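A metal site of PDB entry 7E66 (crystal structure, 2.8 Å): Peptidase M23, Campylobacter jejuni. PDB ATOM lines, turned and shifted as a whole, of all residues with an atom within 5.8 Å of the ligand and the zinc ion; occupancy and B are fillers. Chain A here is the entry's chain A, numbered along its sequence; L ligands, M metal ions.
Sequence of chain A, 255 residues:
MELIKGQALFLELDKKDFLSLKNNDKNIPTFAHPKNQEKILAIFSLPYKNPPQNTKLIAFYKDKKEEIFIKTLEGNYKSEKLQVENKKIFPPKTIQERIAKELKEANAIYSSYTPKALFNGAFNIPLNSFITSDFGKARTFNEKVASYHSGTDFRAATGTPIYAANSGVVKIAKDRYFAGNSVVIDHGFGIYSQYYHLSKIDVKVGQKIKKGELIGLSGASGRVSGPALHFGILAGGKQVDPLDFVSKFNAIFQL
The side-chain hydroxyl (OH) of Tyr 196 lies within hydrogen-bond range of a nitrogen (N3) of the ligand, 2.5 Å away. O5 of the ligand sits at hydrogen-bond distance from NH1 of Arg 176 (2.6 Å). OH of Tyr 110 sits at hydrogen-bond distance from N3 of the ligand, at 2.6 Å. A nitrogen (N3) of the ligand lies close to the side-chain amide nitrogen of Gln 194, 3.0 Å away. An oxygen (O3) of the ligand sits close to the guanidinium group (NE) of Arg 223. NE2 of His 197 sits close to N2 of the ligand (3.2 Å).
Ala 106 touches the ligand. OG of Ser 150 touches C4 of the ligand (3.2 Å). Phe 178 touches the ligand. Gln 239 touches the ligand. Hydrophobic or aromatic side chains that line the ligand: Ala 106, Tyr 110, His 149, Phe 178, Tyr 196, His 197 and His 230. 13 residues have an atom within 4 Å of the ligand: Ala 106, Tyr 110, His 149, Ser 150, Asp 153, Arg 176, Phe 178, Gln 194, Tyr 196, His 197, Arg 223, His 230 and Gln 239.
The zinc ion is bound by O3 of the ligand (1.9 Å), OD1 of Asp 153 (2.1 Å), NE2 of His 149 (2.1 Å) and ND1 of His 230 (2.2 Å). The zinc ion has four donor atoms within binding distance. Slightly farther from the zinc ion lies the side-chain carboxylate (OD2) of Asp 153 (2.6 Å).
Of the 24 residues printed, 3 come within 4 Å of the zinc ion. Along chain A the residues within 4 Å of the zinc ion span positions 149 to 230.
The side-chain carboxylate (OD2) of Asp 153 is in salt-bridge range of the guanidinium group (NH2) of Arg 223 (2.9 Å). The backbone carbonyl oxygen (O) of Ser 133 is in hydrogen-bond range of the backbone NH (N) of Asp 153 (3.0 Å). The backbone carbonyl oxygen (O) of Gly 151 sits at hydrogen-bond distance from a ring nitrogen (ND1) of His 149 (2.7 Å). N of Tyr 196 is in hydrogen-bond range of O of His 230 (3.0 Å). The side-chain hydroxyl (OH) of Tyr 196 is in hydrogen-bond range of the guanidinium group (NH2) of Arg 176, at 3.4 Å. The side-chain hydroxyl (OH) of Tyr 110 sits at hydrogen-bond distance from the side-chain amide nitrogen (NE2) of Gln 194 (3.1 Å). NH1 of Arg 223 is in hydrogen-bond range of O of Ser 225, 3.0 Å away. N of His 197 sits at hydrogen-bond distance from O of Ala 179, 2.9 Å away.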
ATOM      1  N   GLU A 102     -14.945 -22.216   8.493  1.00  0.00           N
ATOM      2  CA  GLU A 102     -16.161 -21.454   8.212  1.00  0.00           C
ATOM      3  C   GLU A 102     -17.416 -22.150   8.758  1.00  0.00           C
ATOM      4  O   GLU A 102     -18.415 -21.500   9.061  1.00  0.00           O
ATOM      5  CB  GLU A 102     -16.300 -21.200   6.709  1.00  0.00           C
ATOM      6  CG  GLU A 102     -15.282 -20.209   6.182  1.00  0.00           C
ATOM      7  CD  GLU A 102     -15.347 -20.004   4.677  1.00  0.00           C
ATOM      8  OE1 GLU A 102     -16.012 -20.802   3.981  1.00  0.00           O
ATOM      9  OE2 GLU A 102     -14.714 -19.056   4.182  1.00  0.00           O
ATOM     10  N   LEU A 103     -17.345 -23.469   8.863  1.00  0.00           N
ATOM     11  CA  LEU A 103     -18.379 -24.264   9.511  1.00  0.00           C
ATOM     12  C   LEU A 103     -18.442 -23.972  11.004  1.00  0.00           C
ATOM     13  O   LEU A 103     -19.518 -23.717  11.553  1.00  0.00           O
ATOM     14  CB  LEU A 103     -18.103 -25.754   9.287  1.00  0.00           C
ATOM     15  CG  LEU A 103     -19.103 -26.735   9.902  1.00  0.00           C
ATOM     16  CD1 LEU A 103     -20.472 -26.585   9.266  1.00  0.00           C
ATOM     17  CD2 LEU A 103     -18.603 -28.160   9.774  1.00  0.00           C
ATOM     18  N   ALA A 106     -19.891 -20.658  11.616  1.00  0.00           N
ATOM     19  CA  ALA A 106     -21.337 -20.705  11.398  1.00  0.00           C
ATOM     20  C   ALA A 106     -22.071 -21.324  12.573  1.00  0.00           C
ATOM     21  O   ALA A 106     -23.054 -20.759  13.066  1.00  0.00           O
ATOM     22  CB  ALA A 106     -21.646 -21.469  10.126  1.00  0.00           C
ATOM     23  N   TYR A 110     -25.062 -19.746  14.781  1.00  0.00           N
ATOM     24  CA  TYR A 110     -26.418 -20.311  14.776  1.00  0.00           C
ATOM     25  C   TYR A 110     -26.849 -20.936  16.094  1.00  0.00           C
ATOM     26  O   TYR A 110     -28.023 -21.264  16.266  1.00  0.00           O
ATOM     27  CB  TYR A 110     -26.570 -21.338  13.650  1.00  0.00           C
ATOM     28  CG  TYR A 110     -26.479 -20.717  12.285  1.00  0.00           C
ATOM     29  CD1 TYR A 110     -27.199 -19.568  11.975  1.00  0.00           C
ATOM     30  CD2 TYR A 110     -25.675 -21.277  11.292  1.00  0.00           C
ATOM     31  CE1 TYR A 110     -27.114 -18.982  10.722  1.00  0.00           C
ATOM     32  CE2 TYR A 110     -25.589 -20.700  10.039  1.00  0.00           C
ATOM     33  CZ  TYR A 110     -26.312 -19.553   9.757  1.00  0.00           C
ATOM     34  OH  TYR A 110     -26.227 -18.977   8.518  1.00  0.00           O
ATOM     35  N   SER A 133     -35.112 -22.021  -8.811  1.00  0.00           N
ATOM     36  CA  SER A 133     -34.860 -23.334  -8.233  1.00  0.00           C
ATOM     37  C   SER A 133     -35.499 -23.427  -6.840  1.00  0.00           C
ATOM     38  O   SER A 133     -35.128 -22.683  -5.940  1.00  0.00           O
ATOM     39  CB  SER A 133     -33.346 -23.587  -8.142  1.00  0.00           C
ATOM     40  OG  SER A 133     -33.052 -24.746  -7.383  1.00  0.00           O
ATOM     41  N   HIS A 149     -31.417 -28.914  -1.871  1.00  0.00           N
ATOM     42  CA  HIS A 149     -31.267 -27.468  -1.935  1.00  0.00           C
ATOM     43  C   HIS A 149     -31.764 -26.867  -0.627  1.00  0.00           C
ATOM     44  O   HIS A 149     -32.952 -26.927  -0.316  1.00  0.00           O
ATOM     45  CB  HIS A 149     -32.053 -26.924  -3.124  1.00  0.00           C
ATOM     46  CG  HIS A 149     -31.725 -25.513  -3.472  1.00  0.00           C
ATOM     47  ND1 HIS A 149     -32.698 -24.596  -3.837  1.00  0.00           N
ATOM     48  CD2 HIS A 149     -30.548 -24.844  -3.500  1.00  0.00           C
ATOM     49  CE1 HIS A 149     -32.124 -23.432  -4.087  1.00  0.00           C
ATOM     50  NE2 HIS A 149     -30.821 -23.559  -3.890  1.00  0.00           N
ATOM     51  N   SER A 150     -30.842 -26.282   0.141  1.00  0.00           N
ATOM     52  CA  SER A 150     -31.140 -25.771   1.479  1.00  0.00           C
ATOM     53  C   SER A 150     -31.835 -24.415   1.501  1.00  0.00           C
ATOM     54  O   SER A 150     -32.177 -23.903   2.564  1.00  0.00           O
ATOM     55  CB  SER A 150     -29.843 -25.663   2.276  1.00  0.00           C
ATOM     56  OG  SER A 150     -28.929 -24.826   1.604  1.00  0.00           O
ATOM     57  N   GLY A 151     -32.033 -23.816   0.321  1.00  0.00           N
ATOM     58  CA  GLY A 151     -32.682 -22.520   0.209  1.00  0.00           C
ATOM     59  C   GLY A 151     -33.515 -22.447  -1.048  1.00  0.00           C
ATOM     60  O   GLY A 151     -33.854 -23.469  -1.623  1.00  0.00           O
ATOM     61  N   THR A 152     -33.839 -21.231  -1.466  1.00  0.00           N
ATOM     62  CA  THR A 152     -34.605 -21.017  -2.689  1.00  0.00           C
ATOM     63  C   THR A 152     -33.875 -19.992  -3.541  1.00  0.00           C
ATOM     64  O   THR A 152     -33.378 -18.984  -3.015  1.00  0.00           O
ATOM     65  CB  THR A 152     -36.061 -20.585  -2.354  1.00  0.00           C
ATOM     66  OG1 THR A 152     -36.940 -21.043  -3.389  1.00  0.00           O
ATOM     67  CG2 THR A 152     -36.192 -19.070  -2.186  1.00  0.00           C
ATOM     68  N   ASP A 153     -33.796 -20.236  -4.845  1.00  0.00           N
ATOM     69  CA  ASP A 153     -33.079 -19.334  -5.739  1.00  0.00           C
ATOM     70  C   ASP A 153     -34.026 -18.472  -6.546  1.00  0.00           C
ATOM     71  O   ASP A 153     -34.904 -18.970  -7.242  1.00  0.00           O
ATOM     72  CB  ASP A 153     -32.167 -20.111  -6.682  1.00  0.00           C
ATOM     73  CG  ASP A 153     -31.106 -20.912  -5.948  1.00  0.00           C
ATOM     74  OD1 ASP A 153     -30.796 -20.580  -4.787  1.00  0.00           O
ATOM     75  OD2 ASP A 153     -30.581 -21.874  -6.544  1.00  0.00           O
ATOM     76  N   ILE A 172     -22.795 -12.337   9.607  1.00  0.00           N
ATOM     77  CA  ILE A 172     -21.815 -12.737   8.609  1.00  0.00           C
ATOM     78  C   ILE A 172     -21.920 -11.778   7.433  1.00  0.00           C
ATOM     79  O   ILE A 172     -23.027 -11.400   7.038  1.00  0.00           O
ATOM     80  CB  ILE A 172     -22.060 -14.182   8.131  1.00  0.00           C
ATOM     81  CG1 ILE A 172     -22.004 -15.160   9.324  1.00  0.00           C
ATOM     82  CG2 ILE A 172     -21.031 -14.582   7.067  1.00  0.00           C
ATOM     83  CD1 ILE A 172     -22.277 -16.603   8.971  1.00  0.00           C
ATOM     84  N   ARG A 176     -17.295 -16.701   1.394  1.00  0.00           N
ATOM     85  CA  ARG A 176     -17.087 -18.031   1.931  1.00  0.00           C
ATOM     86  C   ARG A 176     -17.064 -19.018   0.788  1.00  0.00           C
ATOM     87  O   ARG A 176     -17.434 -18.681  -0.341  1.00  0.00           O
ATOM     88  CB  ARG A 176     -18.190 -18.380   2.913  1.00  0.00           C
ATOM     89  CG  ARG A 176     -18.233 -17.438   4.102  1.00  0.00           C
ATOM     90  CD  ARG A 176     -19.166 -17.955   5.170  1.00  0.00           C
ATOM     91  NE  ARG A 176     -20.558 -17.966   4.724  1.00  0.00           N
ATOM     92  CZ  ARG A 176     -21.571 -18.465   5.416  1.00  0.00           C
ATOM     93  NH1 ARG A 176     -21.366 -19.023   6.598  1.00  0.00           N
ATOM     94  NH2 ARG A 176     -22.799 -18.428   4.909  1.00  0.00           N
ATOM     95  N   PHE A 178     -18.589 -22.335  -0.008  1.00  0.00           N
ATOM     96  CA  PHE A 178     -19.828 -22.793  -0.623  1.00  0.00           C
ATOM     97  C   PHE A 178     -20.802 -21.657  -0.894  1.00  0.00           C
ATOM     98  O   PHE A 178     -21.427 -21.617  -1.954  1.00  0.00           O
ATOM     99  CB  PHE A 178     -20.512 -23.852   0.260  1.00  0.00           C
ATOM    100  CG  PHE A 178     -19.787 -25.165   0.300  1.00  0.00           C
ATOM    101  CD1 PHE A 178     -19.347 -25.769  -0.872  1.00  0.00           C
ATOM    102  CD2 PHE A 178     -19.556 -25.810   1.510  1.00  0.00           C
ATOM    103  CE1 PHE A 178     -18.683 -26.979  -0.833  1.00  0.00           C
ATOM    104  CE2 PHE A 178     -18.891 -27.020   1.549  1.00  0.00           C
ATOM    105  CZ  PHE A 178     -18.455 -27.605   0.377  1.00  0.00           C
ATOM    106  N   ALA A 179     -20.904 -20.727   0.048  1.00  0.00           N
ATOM    107  CA  ALA A 179     -21.930 -19.698   0.023  1.00  0.00           C
ATOM    108  C   ALA A 179     -21.590 -18.473  -0.843  1.00  0.00           C
ATOM    109  O   ALA A 179     -22.464 -17.635  -1.075  1.00  0.00           O
ATOM    110  CB  ALA A 179     -22.254 -19.254   1.441  1.00  0.00           C
ATOM    111  N   VAL A 184     -25.675 -13.000   6.445  1.00  0.00           N
ATOM    112  CA  VAL A 184     -26.599 -13.693   7.343  1.00  0.00           C
ATOM    113  C   VAL A 184     -27.038 -12.732   8.438  1.00  0.00           C
ATOM    114  O   VAL A 184     -26.217 -12.037   9.030  1.00  0.00           O
ATOM    115  CB  VAL A 184     -25.937 -14.941   7.955  1.00  0.00           C
ATOM    116  CG1 VAL A 184     -26.879 -15.619   8.930  1.00  0.00           C
ATOM    117  CG2 VAL A 184     -25.520 -15.906   6.865  1.00  0.00           C
ATOM    118  N   GLN A 194     -30.581 -15.658   5.155  1.00  0.00           N
ATOM    119  CA  GLN A 194     -29.322 -15.890   4.469  1.00  0.00           C
ATOM    120  C   GLN A 194     -29.410 -15.407   3.031  1.00  0.00           C
ATOM    121  O   GLN A 194     -30.411 -15.643   2.356  1.00  0.00           O
ATOM    122  CB  GLN A 194     -28.999 -17.379   4.491  1.00  0.00           C
ATOM    123  CG  GLN A 194     -29.014 -17.998   5.884  1.00  0.00           C
ATOM    124  CD  GLN A 194     -29.101 -19.512   5.866  1.00  0.00           C
ATOM    125  OE1 GLN A 194     -29.636 -20.110   4.929  1.00  0.00           O
ATOM    126  NE2 GLN A 194     -28.579 -20.156   6.905  1.00  0.00           N
ATOM    127  N   TYR A 196     -26.907 -15.358  -0.396  1.00  0.00           N
ATOM    128  CA  TYR A 196     -25.652 -15.920  -0.877  1.00  0.00           C
ATOM    129  C   TYR A 196     -25.329 -15.573  -2.324  1.00  0.00           C
ATOM    130  O   TYR A 196     -26.187 -15.124  -3.083  1.00  0.00           O
ATOM    131  CB  TYR A 196     -25.653 -17.445  -0.731  1.00  0.00           C
ATOM    132  CG  TYR A 196     -25.741 -17.986   0.687  1.00  0.00           C
ATOM    133  CD1 TYR A 196     -25.524 -17.172   1.796  1.00  0.00           C
ATOM    134  CD2 TYR A 196     -26.008 -19.333   0.901  1.00  0.00           C
ATOM    135  CE1 TYR A 196     -25.597 -17.676   3.082  1.00  0.00           C
ATOM    136  CE2 TYR A 196     -26.079 -19.848   2.187  1.00  0.00           C
ATOM    137  CZ  TYR A 196     -25.875 -19.024   3.267  1.00  0.00           C
ATOM    138  OH  TYR A 196     -25.954 -19.529   4.545  1.00  0.00           O
ATOM    139  N   HIS A 197     -24.059 -15.812  -2.682  1.00  0.00           N
ATOM    140  CA  HIS A 197     -23.551 -15.640  -4.041  1.00  0.00           C
ATOM    141  C   HIS A 197     -23.685 -14.219  -4.532  1.00  0.00           C
ATOM    142  O   HIS A 197     -23.888 -13.985  -5.721  1.00  0.00           O
ATOM    143  CB  HIS A 197     -24.241 -16.618  -4.982  1.00  0.00           C
ATOM    144  CG  HIS A 197     -24.360 -17.991  -4.421  1.00  0.00           C
ATOM    145  ND1 HIS A 197     -23.258 -18.782  -4.173  1.00  0.00           N
ATOM    146  CD2 HIS A 197     -25.434 -18.695  -4.007  1.00  0.00           C
ATOM    147  CE1 HIS A 197     -23.653 -19.925  -3.657  1.00  0.00           C
ATOM    148  NE2 HIS A 197     -24.972 -19.900  -3.547  1.00  0.00           N
ATOM    149  N   ARG A 223     -20.858 -19.880  -7.049  1.00  0.00           N
ATOM    150  CA  ARG A 223     -21.992 -20.533  -7.677  1.00  0.00           C
ATOM    151  C   ARG A 223     -21.558 -21.073  -9.031  1.00  0.00           C
ATOM    152  O   ARG A 223     -20.988 -20.339  -9.841  1.00  0.00           O
ATOM    153  CB  ARG A 223     -23.133 -19.538  -7.863  1.00  0.00           C
ATOM    154  CG  ARG A 223     -24.483 -20.175  -8.162  1.00  0.00           C
ATOM    155  CD  ARG A 223     -25.636 -19.281  -7.721  1.00  0.00           C
ATOM    156  NE  ARG A 223     -26.908 -19.986  -7.689  1.00  0.00           N
ATOM    157  CZ  ARG A 223     -27.649 -20.289  -8.761  1.00  0.00           C
ATOM    158  NH1 ARG A 223     -27.255 -19.947  -9.981  1.00  0.00           N
ATOM    159  NH2 ARG A 223     -28.800 -20.937  -8.601  1.00  0.00           N
ATOM    160  N   SER A 225     -23.693 -22.603 -11.301  1.00  0.00           N
ATOM    161  CA  SER A 225     -24.768 -22.537 -12.296  1.00  0.00           C
ATOM    162  C   SER A 225     -25.294 -21.115 -12.547  1.00  0.00           C
ATOM    163  O   SER A 225     -26.501 -20.903 -12.688  1.00  0.00           O
ATOM    164  CB  SER A 225     -25.905 -23.474 -11.884  1.00  0.00           C
ATOM    165  OG  SER A 225     -26.307 -23.223 -10.539  1.00  0.00           O
ATOM    166  N   LEU A 229     -29.856 -15.178  -6.870  1.00  0.00           N
ATOM    167  CA  LEU A 229     -29.859 -15.007  -5.427  1.00  0.00           C
ATOM    168  C   LEU A 229     -30.308 -16.305  -4.773  1.00  0.00           C
ATOM    169  O   LEU A 229     -31.319 -16.884  -5.172  1.00  0.00           O
ATOM    170  CB  LEU A 229     -30.797 -13.896  -4.962  1.00  0.00           C
ATOM    171  CG  LEU A 229     -30.844 -13.775  -3.426  1.00  0.00           C
ATOM    172  CD1 LEU A 229     -29.631 -13.004  -2.913  1.00  0.00           C
ATOM    173  CD2 LEU A 229     -32.132 -13.147  -2.938  1.00  0.00           C
ATOM    174  N   HIS A 230     -29.567 -16.730  -3.754  1.00  0.00           N
ATOM    175  CA  HIS A 230     -29.963 -17.852  -2.917  1.00  0.00           C
ATOM    176  C   HIS A 230     -30.391 -17.301  -1.568  1.00  0.00           C
ATOM    177  O   HIS A 230     -29.584 -16.755  -0.820  1.00  0.00           O
ATOM    178  CB  HIS A 230     -28.789 -18.811  -2.761  1.00  0.00           C
ATOM    179  CG  HIS A 230     -29.055 -19.925  -1.798  1.00  0.00           C
ATOM    180  ND1 HIS A 230     -29.259 -21.224  -2.208  1.00  0.00           N
ATOM    181  CD2 HIS A 230     -29.140 -19.947  -0.449  1.00  0.00           C
ATOM    182  CE1 HIS A 230     -29.452 -21.995  -1.159  1.00  0.00           C
ATOM    183  NE2 HIS A 230     -29.388 -21.245  -0.074  1.00  0.00           N
ATOM    184  N   LEU A 234     -32.774 -20.104   8.490  1.00  0.00           N
ATOM    185  CA  LEU A 234     -32.471 -21.048   9.544  1.00  0.00           C
ATOM    186  C   LEU A 234     -33.360 -20.709  10.732  1.00  0.00           C
ATOM    187  O   LEU A 234     -33.388 -19.550  11.165  1.00  0.00           O
ATOM    188  CB  LEU A 234     -31.002 -20.992   9.936  1.00  0.00           C
ATOM    189  CG  LEU A 234     -30.522 -22.165  10.804  1.00  0.00           C
ATOM    190  CD1 LEU A 234     -29.083 -22.529  10.464  1.00  0.00           C
ATOM    191  CD2 LEU A 234     -30.659 -21.854  12.291  1.00  0.00           C
ATOM    192  N   GLN A 239     -32.035 -25.502   8.657  1.00  0.00           N
ATOM    193  CA  GLN A 239     -32.435 -24.923   7.372  1.00  0.00           C
ATOM    194  C   GLN A 239     -33.863 -25.361   7.103  1.00  0.00           C
ATOM    195  O   GLN A 239     -34.191 -26.543   7.233  1.00  0.00           O
ATOM    196  CB  GLN A 239     -31.546 -25.425   6.226  1.00  0.00           C
ATOM    197  CG  GLN A 239     -30.104 -24.957   6.249  1.00  0.00           C
ATOM    198  CD  GLN A 239     -29.932 -23.440   6.276  1.00  0.00           C
ATOM    199  OE1 GLN A 239     -28.972 -22.935   6.866  1.00  0.00           O
ATOM    200  NE2 GLN A 239     -30.848 -22.709   5.637  1.00  0.00           N
HETATM  201  C1  LIG L   1     -26.678 -23.286  -4.008  1.00  0.00           C
HETATM  202  C2  LIG L   1     -24.203 -23.372   2.517  1.00  0.00           C
HETATM  203  N1  LIG L   1     -26.244 -24.036  -1.532  1.00  0.00           N
HETATM  204  N2  LIG L   1     -27.257 -22.021  -4.406  1.00  0.00           N
HETATM  205  C3  LIG L   1     -25.791 -23.380  -2.754  1.00  0.00           C
HETATM  206  C4  LIG L   1     -25.834 -24.608   0.984  1.00  0.00           C
HETATM  207  O1  LIG L   1     -24.402 -23.323  -0.386  1.00  0.00           O
HETATM  208  S1  LIG L   1     -24.373 -21.794   6.275  1.00  0.00           S
HETATM  209  C5  LIG L   1     -25.419 -23.936  -0.326  1.00  0.00           C
HETATM  210  O2  LIG L   1     -26.874 -24.252  -4.666  1.00  0.00           O
HETATM  211  O3  LIG L   1     -28.058 -21.947  -5.560  1.00  0.00           O
HETATM  212  O4  LIG L   1     -24.189 -22.903   7.480  1.00  0.00           O
HETATM  213  N3  LIG L   1     -25.620 -20.691   6.680  1.00  0.00           N
HETATM  214  O5  LIG L   1     -22.956 -20.979   6.062  1.00  0.00           O
HETATM  215  C6  LIG L   1     -25.472 -23.898   2.309  1.00  0.00           C
HETATM  216  C7  LIG L   1     -26.407 -23.796   3.340  1.00  0.00           C
HETATM  217  C8  LIG L   1     -26.085 -23.159   4.537  1.00  0.00           C
HETATM  218  C9  LIG L   1     -24.822 -22.624   4.723  1.00  0.00           C
HETATM  219  C10 LIG L   1     -23.879 -22.735   3.699  1.00  0.00           C
HETATM  220 ZN    ZN M   1     -29.397 -22.030  -4.234  1.00  0.00          ZN
